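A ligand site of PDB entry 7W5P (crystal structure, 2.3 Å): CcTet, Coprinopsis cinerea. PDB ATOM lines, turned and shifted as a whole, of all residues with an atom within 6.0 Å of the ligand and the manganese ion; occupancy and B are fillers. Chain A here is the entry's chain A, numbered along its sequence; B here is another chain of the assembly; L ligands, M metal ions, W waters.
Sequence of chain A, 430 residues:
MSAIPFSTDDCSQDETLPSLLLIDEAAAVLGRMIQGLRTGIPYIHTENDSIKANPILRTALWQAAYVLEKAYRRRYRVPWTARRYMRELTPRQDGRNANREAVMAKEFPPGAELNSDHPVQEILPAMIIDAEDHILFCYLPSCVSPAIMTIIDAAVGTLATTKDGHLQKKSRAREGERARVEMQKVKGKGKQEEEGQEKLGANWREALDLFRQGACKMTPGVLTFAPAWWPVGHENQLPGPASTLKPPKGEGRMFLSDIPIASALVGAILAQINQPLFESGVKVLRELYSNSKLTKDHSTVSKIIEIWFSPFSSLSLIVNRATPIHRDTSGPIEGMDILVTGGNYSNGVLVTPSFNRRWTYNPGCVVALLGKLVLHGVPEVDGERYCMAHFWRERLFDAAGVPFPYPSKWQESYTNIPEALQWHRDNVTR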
ATOM      1  N   TRP A 204     -16.568 -18.557  18.519  1.00  0.00           N
ATOM      2  CA  TRP A 204     -16.347 -19.924  17.994  1.00  0.00           C
ATOM      3  C   TRP A 204     -17.607 -20.805  18.061  1.00  0.00           C
ATOM      4  O   TRP A 204     -17.729 -21.603  17.287  1.00  0.00           O
ATOM      5  CB  TRP A 204     -15.095 -20.575  18.594  1.00  0.00           C
ATOM      6  CG  TRP A 204     -15.183 -20.972  20.024  1.00  0.00           C
ATOM      7  CD1 TRP A 204     -14.663 -20.310  21.080  1.00  0.00           C
ATOM      8  CD2 TRP A 204     -15.859 -22.095  20.575  1.00  0.00           C
ATOM      9  NE1 TRP A 204     -14.945 -20.939  22.238  1.00  0.00           N
ATOM     10  CE2 TRP A 204     -15.661 -22.053  21.966  1.00  0.00           C
ATOM     11  CE3 TRP A 204     -16.566 -23.143  20.048  1.00  0.00           C
ATOM     12  CZ2 TRP A 204     -16.138 -23.023  22.835  1.00  0.00           C
ATOM     13  CZ3 TRP A 204     -17.066 -24.069  20.895  1.00  0.00           C
ATOM     14  CH2 TRP A 204     -16.840 -24.023  22.260  1.00  0.00           C
ATOM     15  N   ARG A 205     -18.480 -20.581  19.003  1.00  0.00           N
ATOM     16  CA  ARG A 205     -19.721 -21.374  19.145  1.00  0.00           C
ATOM     17  C   ARG A 205     -20.642 -21.207  17.943  1.00  0.00           C
ATOM     18  O   ARG A 205     -21.424 -22.018  17.707  1.00  0.00           O
ATOM     19  CB  ARG A 205     -20.407 -21.031  20.471  1.00  0.00           C
ATOM     20  CG  ARG A 205     -19.575 -21.369  21.676  1.00  0.00           C
ATOM     21  CD  ARG A 205     -20.362 -20.945  22.840  1.00  0.00           C
ATOM     22  NE  ARG A 205     -19.700 -21.125  24.067  1.00  0.00           N
ATOM     23  CZ  ARG A 205     -19.492 -22.195  24.770  1.00  0.00           C
ATOM     24  NH1 ARG A 205     -19.908 -23.362  24.394  1.00  0.00           N
ATOM     25  NH2 ARG A 205     -18.883 -22.077  25.885  1.00  0.00           N
ATOM     26  N   ILE A 318     -27.321 -26.946  20.427  1.00  0.00           N
ATOM     27  CA  ILE A 318     -26.353 -26.776  19.356  1.00  0.00           C
ATOM     28  C   ILE A 318     -26.716 -27.773  18.253  1.00  0.00           C
ATOM     29  O   ILE A 318     -26.552 -28.983  18.424  1.00  0.00           O
ATOM     30  CB  ILE A 318     -24.922 -26.979  19.853  1.00  0.00           C
ATOM     31  CG1 ILE A 318     -24.631 -26.046  21.029  1.00  0.00           C
ATOM     32  CG2 ILE A 318     -23.919 -26.758  18.740  1.00  0.00           C
ATOM     33  CD1 ILE A 318     -24.707 -26.718  22.388  1.00  0.00           C
ATOM     34  N   ARG A 321     -23.400 -28.808  14.591  1.00  0.00           N
ATOM     35  CA  ARG A 321     -22.122 -28.125  14.756  1.00  0.00           C
ATOM     36  C   ARG A 321     -21.134 -29.071  15.419  1.00  0.00           C
ATOM     37  O   ARG A 321     -21.427 -29.626  16.481  1.00  0.00           O
ATOM     38  CB  ARG A 321     -22.286 -26.838  15.586  1.00  0.00           C
ATOM     39  CG  ARG A 321     -21.112 -25.878  15.482  1.00  0.00           C
ATOM     40  CD  ARG A 321     -20.940 -25.046  16.747  1.00  0.00           C
ATOM     41  NE  ARG A 321     -20.489 -25.852  17.885  1.00  0.00           N
ATOM     42  CZ  ARG A 321     -20.678 -25.527  19.157  1.00  0.00           C
ATOM     43  NH1 ARG A 321     -21.327 -24.402  19.474  1.00  0.00           N
ATOM     44  NH2 ARG A 321     -20.237 -26.324  20.124  1.00  0.00           N
ATOM     45  N   ALA A 322     -19.991 -29.269  14.785  1.00  0.00           N
ATOM     46  CA  ALA A 322     -18.852 -29.873  15.447  1.00  0.00           C
ATOM     47  C   ALA A 322     -18.366 -28.961  16.564  1.00  0.00           C
ATOM     48  O   ALA A 322     -18.629 -27.750  16.573  1.00  0.00           O
ATOM     49  CB  ALA A 322     -17.733 -30.156  14.452  1.00  0.00           C
ATOM     50  N   THR A 323     -17.626 -29.530  17.516  1.00  0.00           N
ATOM     51  CA  THR A 323     -17.192 -28.790  18.695  1.00  0.00           C
ATOM     52  C   THR A 323     -15.690 -28.977  18.871  1.00  0.00           C
ATOM     53  O   THR A 323     -15.228 -30.118  19.090  1.00  0.00           O
ATOM     54  CB  THR A 323     -17.958 -29.265  19.936  1.00  0.00           C
ATOM     55  OG1 THR A 323     -19.348 -28.986  19.769  1.00  0.00           O
ATOM     56  CG2 THR A 323     -17.447 -28.557  21.168  1.00  0.00           C
ATOM     57  N   HIS A 326     -12.067 -27.504  23.946  1.00  0.00           N
ATOM     58  CA  HIS A 326     -12.222 -26.257  24.682  1.00  0.00           C
ATOM     59  C   HIS A 326     -12.529 -26.572  26.133  1.00  0.00           C
ATOM     60  O   HIS A 326     -12.949 -27.689  26.472  1.00  0.00           O
ATOM     61  CB  HIS A 326     -13.344 -25.413  24.078  1.00  0.00           C
ATOM     62  CG  HIS A 326     -14.716 -25.939  24.382  1.00  0.00           C
ATOM     63  ND1 HIS A 326     -15.231 -27.068  23.773  1.00  0.00           N
ATOM     64  CD2 HIS A 326     -15.658 -25.528  25.261  1.00  0.00           C
ATOM     65  CE1 HIS A 326     -16.432 -27.311  24.250  1.00  0.00           C
ATOM     66  NE2 HIS A 326     -16.718 -26.394  25.151  1.00  0.00           N
ATOM     67  N   ARG A 327     -12.367 -25.569  26.984  1.00  0.00           N
ATOM     68  CA  ARG A 327     -12.942 -25.536  28.312  1.00  0.00           C
ATOM     69  C   ARG A 327     -13.988 -24.434  28.345  1.00  0.00           C
ATOM     70  O   ARG A 327     -13.769 -23.362  27.760  1.00  0.00           O
ATOM     71  CB  ARG A 327     -11.884 -25.272  29.401  1.00  0.00           C
ATOM     72  CG  ARG A 327     -11.007 -26.452  29.805  1.00  0.00           C
ATOM     73  CD  ARG A 327     -10.073 -26.037  30.954  1.00  0.00           C
ATOM     74  NE  ARG A 327      -8.904 -26.917  31.109  1.00  0.00           N
ATOM     75  CZ  ARG A 327      -7.738 -26.723  30.515  1.00  0.00           C
ATOM     76  NH1 ARG A 327      -7.565 -25.671  29.709  1.00  0.00           N
ATOM     77  NH2 ARG A 327      -6.734 -27.572  30.722  1.00  0.00           N
ATOM     78  N   ASP A 328     -15.118 -24.704  28.992  1.00  0.00           N
ATOM     79  CA  ASP A 328     -16.121 -23.657  29.207  1.00  0.00           C
ATOM     80  C   ASP A 328     -15.693 -22.850  30.429  1.00  0.00           C
ATOM     81  O   ASP A 328     -15.637 -23.374  31.544  1.00  0.00           O
ATOM     82  CB  ASP A 328     -17.508 -24.273  29.394  1.00  0.00           C
ATOM     83  CG  ASP A 328     -17.907 -25.181  28.245  1.00  0.00           C
ATOM     84  OD1 ASP A 328     -18.125 -24.679  27.114  1.00  0.00           O
ATOM     85  OD2 ASP A 328     -18.017 -26.414  28.478  1.00  0.00           O
ATOM     86  N   LEU A 339     -24.054 -32.920  29.102  1.00  0.00           N
ATOM     87  CA  LEU A 339     -24.249 -32.927  27.657  1.00  0.00           C
ATOM     88  C   LEU A 339     -25.089 -34.135  27.272  1.00  0.00           C
ATOM     89  O   LEU A 339     -24.857 -35.244  27.751  1.00  0.00           O
ATOM     90  CB  LEU A 339     -22.917 -32.982  26.922  1.00  0.00           C
ATOM     91  CG  LEU A 339     -21.864 -31.961  27.321  1.00  0.00           C
ATOM     92  CD1 LEU A 339     -20.525 -32.349  26.725  1.00  0.00           C
ATOM     93  CD2 LEU A 339     -22.306 -30.574  26.851  1.00  0.00           C
ATOM     94  N   VAL A 340     -26.071 -33.896  26.402  1.00  0.00           N
ATOM     95  CA  VAL A 340     -26.896 -34.949  25.806  1.00  0.00           C
ATOM     96  C   VAL A 340     -26.797 -34.775  24.299  1.00  0.00           C
ATOM     97  O   VAL A 340     -27.064 -33.691  23.779  1.00  0.00           O
ATOM     98  CB  VAL A 340     -28.362 -34.873  26.265  1.00  0.00           C
ATOM     99  CG1 VAL A 340     -29.162 -36.038  25.713  1.00  0.00           C
ATOM    100  CG2 VAL A 340     -28.449 -34.829  27.795  1.00  0.00           C
ATOM    101  N   THR A 341     -26.387 -35.824  23.595  1.00  0.00           N
ATOM    102  CA  THR A 341     -26.250 -35.755  22.149  1.00  0.00           C
ATOM    103  C   THR A 341     -27.286 -36.653  21.475  1.00  0.00           C
ATOM    104  O   THR A 341     -27.673 -37.696  22.008  1.00  0.00           O
ATOM    105  CB  THR A 341     -24.831 -36.141  21.712  1.00  0.00           C
ATOM    106  OG1 THR A 341     -24.691 -35.959  20.292  1.00  0.00           O
ATOM    107  CG2 THR A 341     -24.502 -37.578  22.074  1.00  0.00           C
ATOM    108  N   LEU A 350     -16.266 -38.098  21.537  1.00  0.00           N
ATOM    109  CA  LEU A 350     -15.939 -36.991  22.430  1.00  0.00           C
ATOM    110  C   LEU A 350     -14.510 -37.178  22.911  1.00  0.00           C
ATOM    111  O   LEU A 350     -14.148 -38.249  23.394  1.00  0.00           O
ATOM    112  CB  LEU A 350     -16.914 -36.906  23.609  1.00  0.00           C
ATOM    113  CG  LEU A 350     -16.716 -35.682  24.522  1.00  0.00           C
ATOM    114  CD1 LEU A 350     -18.020 -34.929  24.742  1.00  0.00           C
ATOM    115  CD2 LEU A 350     -16.120 -36.094  25.854  1.00  0.00           C
ATOM    116  N   TYR A 361     -19.564 -41.421  21.287  1.00  0.00           N
ATOM    117  CA  TYR A 361     -20.486 -40.321  21.591  1.00  0.00           C
ATOM    118  C   TYR A 361     -21.635 -40.343  20.583  1.00  0.00           C
ATOM    119  O   TYR A 361     -21.777 -39.424  19.763  1.00  0.00           O
ATOM    120  CB  TYR A 361     -19.725 -38.992  21.577  1.00  0.00           C
ATOM    121  CG  TYR A 361     -20.427 -37.823  22.203  1.00  0.00           C
ATOM    122  CD1 TYR A 361     -20.819 -37.831  23.543  1.00  0.00           C
ATOM    123  CD2 TYR A 361     -20.680 -36.661  21.465  1.00  0.00           C
ATOM    124  CE1 TYR A 361     -21.447 -36.750  24.115  1.00  0.00           C
ATOM    125  CE2 TYR A 361     -21.309 -35.583  22.027  1.00  0.00           C
ATOM    126  CZ  TYR A 361     -21.693 -35.628  23.347  1.00  0.00           C
ATOM    127  OH  TYR A 361     -22.322 -34.528  23.913  1.00  0.00           O
ATOM    128  N   GLY A 371     -16.973 -28.759  33.239  1.00  0.00           N
ATOM    129  CA  GLY A 371     -16.674 -28.101  31.974  1.00  0.00           C
ATOM    130  C   GLY A 371     -15.566 -27.067  32.077  1.00  0.00           C
ATOM    131  O   GLY A 371     -14.880 -26.797  31.092  1.00  0.00           O
ATOM    132  N   HIS A 376     -12.661 -30.719  26.224  1.00  0.00           N
ATOM    133  CA  HIS A 376     -13.533 -31.626  25.501  1.00  0.00           C
ATOM    134  C   HIS A 376     -13.889 -31.034  24.146  1.00  0.00           C
ATOM    135  O   HIS A 376     -14.009 -29.812  24.007  1.00  0.00           O
ATOM    136  CB  HIS A 376     -14.807 -31.942  26.286  1.00  0.00           C
ATOM    137  CG  HIS A 376     -15.614 -30.732  26.626  1.00  0.00           C
ATOM    138  ND1 HIS A 376     -15.228 -29.822  27.585  1.00  0.00           N
ATOM    139  CD2 HIS A 376     -16.810 -30.301  26.154  1.00  0.00           C
ATOM    140  CE1 HIS A 376     -16.144 -28.871  27.684  1.00  0.00           C
ATOM    141  NE2 HIS A 376     -17.114 -29.132  26.827  1.00  0.00           N
ATOM    142  N   VAL A 378     -15.891 -32.342  20.071  1.00  0.00           N
ATOM    143  CA  VAL A 378     -16.646 -33.340  19.310  1.00  0.00           C
ATOM    144  C   VAL A 378     -16.423 -33.113  17.824  1.00  0.00           C
ATOM    145  O   VAL A 378     -16.883 -32.086  17.282  1.00  0.00           O
ATOM    146  CB  VAL A 378     -18.144 -33.288  19.664  1.00  0.00           C
ATOM    147  CG1 VAL A 378     -18.905 -34.333  18.857  1.00  0.00           C
ATOM    148  CG2 VAL A 378     -18.356 -33.494  21.153  1.00  0.00           C
ATOM    149  N   ARG A 385     -26.712 -34.035  13.775  1.00  0.00           N
ATOM    150  CA  ARG A 385     -26.528 -34.167  15.213  1.00  0.00           C
ATOM    151  C   ARG A 385     -26.972 -32.875  15.895  1.00  0.00           C
ATOM    152  O   ARG A 385     -26.883 -31.796  15.313  1.00  0.00           O
ATOM    153  CB  ARG A 385     -25.055 -34.470  15.557  1.00  0.00           C
ATOM    154  CG  ARG A 385     -24.724 -34.486  17.046  1.00  0.00           C
ATOM    155  CD  ARG A 385     -23.265 -34.867  17.280  1.00  0.00           C
ATOM    156  NE  ARG A 385     -22.409 -33.697  17.379  1.00  0.00           N
ATOM    157  CZ  ARG A 385     -22.192 -33.032  18.513  1.00  0.00           C
ATOM    158  NH1 ARG A 385     -22.771 -33.433  19.634  1.00  0.00           N
ATOM    159  NH2 ARG A 385     -21.396 -31.975  18.530  1.00  0.00           N
ATOM    160  N   TYR A 386     -27.479 -33.021  17.115  1.00  0.00           N
ATOM    161  CA  TYR A 386     -27.745 -31.917  18.006  1.00  0.00           C
ATOM    162  C   TYR A 386     -27.223 -32.257  19.407  1.00  0.00           C
ATOM    163  O   TYR A 386     -27.057 -33.431  19.757  1.00  0.00           O
ATOM    164  CB  TYR A 386     -29.240 -31.571  18.063  1.00  0.00           C
ATOM    165  CG  TYR A 386     -30.094 -32.669  18.648  1.00  0.00           C
ATOM    166  CD1 TYR A 386     -30.622 -33.669  17.851  1.00  0.00           C
ATOM    167  CD2 TYR A 386     -30.362 -32.705  20.015  1.00  0.00           C
ATOM    168  CE1 TYR A 386     -31.401 -34.675  18.388  1.00  0.00           C
ATOM    169  CE2 TYR A 386     -31.140 -33.698  20.558  1.00  0.00           C
ATOM    170  CZ  TYR A 386     -31.660 -34.683  19.744  1.00  0.00           C
ATOM    171  OH  TYR A 386     -32.439 -35.688  20.280  1.00  0.00           O
ATOM    172  N   CYS A 387     -26.959 -31.209  20.189  1.00  0.00           N
ATOM    173  CA  CYS A 387     -26.461 -31.353  21.551  1.00  0.00           C
ATOM    174  C   CYS A 387     -27.228 -30.417  22.473  1.00  0.00           C
ATOM    175  O   CYS A 387     -27.443 -29.253  22.132  1.00  0.00           O
ATOM    176  CB  CYS A 387     -24.951 -31.077  21.630  1.00  0.00           C
ATOM    177  SG  CYS A 387     -24.325 -30.798  23.315  1.00  0.00           S
ATOM    178  N   ALA A 389     -26.711 -28.839  26.100  1.00  0.00           N
ATOM    179  CA  ALA A 389     -25.703 -28.580  27.111  1.00  0.00           C
ATOM    180  C   ALA A 389     -26.379 -27.866  28.283  1.00  0.00           C
ATOM    181  O   ALA A 389     -26.906 -26.767  28.107  1.00  0.00           O
ATOM    182  CB  ALA A 389     -24.564 -27.736  26.552  1.00  0.00           C
ATOM    183  P   6MA B   6     -20.289 -16.476  27.847  1.00  0.00           P
ATOM    184  OP1 6MA B   6     -20.813 -16.167  29.175  1.00  0.00           O
ATOM    185  OP2 6MA B   6     -19.320 -17.517  27.423  1.00  0.00           O
ATOM    186  O5' 6MA B   6     -21.523 -16.719  26.879  1.00  0.00           O
ATOM    187  C5' 6MA B   6     -21.421 -16.716  25.395  1.00  0.00           C
ATOM    188  C4' 6MA B   6     -22.431 -17.711  24.940  1.00  0.00           C
ATOM    189  O4' 6MA B   6     -21.865 -18.975  25.186  1.00  0.00           O
ATOM    190  C3' 6MA B   6     -23.775 -17.681  25.568  1.00  0.00           C
ATOM    191  O3' 6MA B   6     -24.904 -17.689  24.733  1.00  0.00           O
ATOM    192  C2' 6MA B   6     -23.795 -18.908  26.465  1.00  0.00           C
ATOM    193  C1' 6MA B   6     -22.814 -19.852  25.817  1.00  0.00           C
ATOM    194  N9  6MA B   6     -22.280 -20.691  26.808  1.00  0.00           N
ATOM    195  C8  6MA B   6     -21.648 -20.266  27.959  1.00  0.00           C
ATOM    196  N7  6MA B   6     -21.239 -21.251  28.737  1.00  0.00           N
ATOM    197  C5  6MA B   6     -21.623 -22.411  28.048  1.00  0.00           C
ATOM    198  C6  6MA B   6     -21.436 -23.740  28.404  1.00  0.00           C
ATOM    199  N1  6MA B   6     -21.951 -24.692  27.462  1.00  0.00           N
ATOM    200  C2  6MA B   6     -22.561 -24.212  26.343  1.00  0.00           C
ATOM    201  N3  6MA B   6     -22.723 -22.925  26.020  1.00  0.00           N
ATOM    202  C4  6MA B   6     -22.258 -22.074  26.883  1.00  0.00           C
ATOM    203  N6  6MA B   6     -20.833 -24.210  29.552  1.00  0.00           N
ATOM    204  C1  6MA B   6     -21.026 -25.648  29.682  1.00  0.00           C
HETATM  205  C1  LIG L   1     -20.122 -26.991  23.977  1.00  0.00           C
HETATM  206  C2  LIG L   1     -19.972 -28.517  24.115  1.00  0.00           C
HETATM  207  C3  LIG L   1     -20.514 -30.771  23.176  1.00  0.00           C
HETATM  208  C4  LIG L   1     -21.163 -31.315  21.885  1.00  0.00           C
HETATM  209  O1  LIG L   1     -19.608 -26.215  24.828  1.00  0.00           O
HETATM  210  O2  LIG L   1     -20.783 -26.526  23.017  1.00  0.00           O
HETATM  211  O3  LIG L   1     -19.340 -28.960  25.082  1.00  0.00           O
HETATM  212  O4  LIG L   1     -21.648 -32.464  21.935  1.00  0.00           O
HETATM  213  N1  LIG L   1     -20.567 -29.292  23.179  1.00  0.00           N
HETATM  214  O5  LIG L   1     -21.154 -30.561  20.889  1.00  0.00           O
HETATM  215 MN    MN M   1     -18.399 -27.258  26.311  1.00  0.00          MN
HETATM  216  O   HOH W   1     -20.377 -27.451  27.109  1.00  0.00           O
HETATM  217  O   HOH W   2     -21.710 -23.912  22.144  1.00  0.00           O
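Residues that only touch the ligand: Val 378 (3.5 Å), Leu 339 (3.8 Å), 6MA 6 of chain B (3.8 Å) and Ile 318 (3.98 Å).
Hydrophobic or aromatic side chains within 4 Å of the ligand: Ile 318, His 326, Leu 339, Tyr 361, His 376 and Val 378.
Of the 22 residues printed, 13 come within 4 Å of the ligand.
The nearest printed residue that does not touch the ligand is Trp 204 (4.4 Å).
Water W2 lies within hydrogen-bond range of the guanidinium group of Arg 321 (2.7 Å), an oxygen (O2) of the ligand (2.9 Å) and the guanidinium group of Arg 205 (2.9 Å).
O of Thr 323 lies within hydrogen-bond range of N of Val 378 (2.5 Å).
The side-chain hydroxyl of Thr 323 is in hydrogen-bond range of the guanidinium group of Arg 321, 2.8 Å away.
The guanidinium group of Arg 205 lies within salt-bridge range of the side-chain carboxylate of Asp 328 (3.0 Å).
O of Gly 371 is in hydrogen-bond range of N of Asp 328, 3.0 Å away.
OG1 of Thr 341 sits at hydrogen-bond distance from NH1 of Arg 385 (3.2 Å).
O of Arg 205 is in hydrogen-bond range of NH1 of Arg 321, at 3.0 Å.
The backbone NH (N) of Cys 387 lies within hydrogen-bond range of the backbone carbonyl oxygen (O) of Ile 318, at 2.9 Å.
O4' of 6MA 6 of chain B is in hydrogen-bond range of NE of Arg 205 (3.2 Å).
Of the 22 residues printed, 3 come within 4 Å of the manganese ion.
The side-chain hydroxyl (OG1) of Thr 323 is in hydrogen-bond range of an oxygen (O5) of the ligand (2.6 Å).
The guanidinium group of Arg 385 is in salt-bridge range of an oxygen (O4) of the ligand (2.7 Å).
NH2 of Arg 321 is in salt-bridge range of O2 of the ligand, 3.0 Å away.
NH1 of Arg 205 is in salt-bridge range of O2 of the ligand.
O4 of the ligand is in hydrogen-bond range of SG of Cys 387, at 3.4 Å.
An oxygen (O4) of the ligand is in hydrogen-bond range of the side-chain hydroxyl of Tyr 361 (2.9 Å).
The manganese ion is bound by water W1 (2.1 Å), O1 of the ligand (2.2 Å), NE2 of His 326 (2.2 Å), O3 of the ligand (2.3 Å), NE2 of His 376 (2.3 Å) and OD2 of Asp 328 (2.4 Å).
The manganese ion has six donor atoms within binding distance.
Slightly farther from the manganese ion lies OD1 of Asp 328 (2.7 Å).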
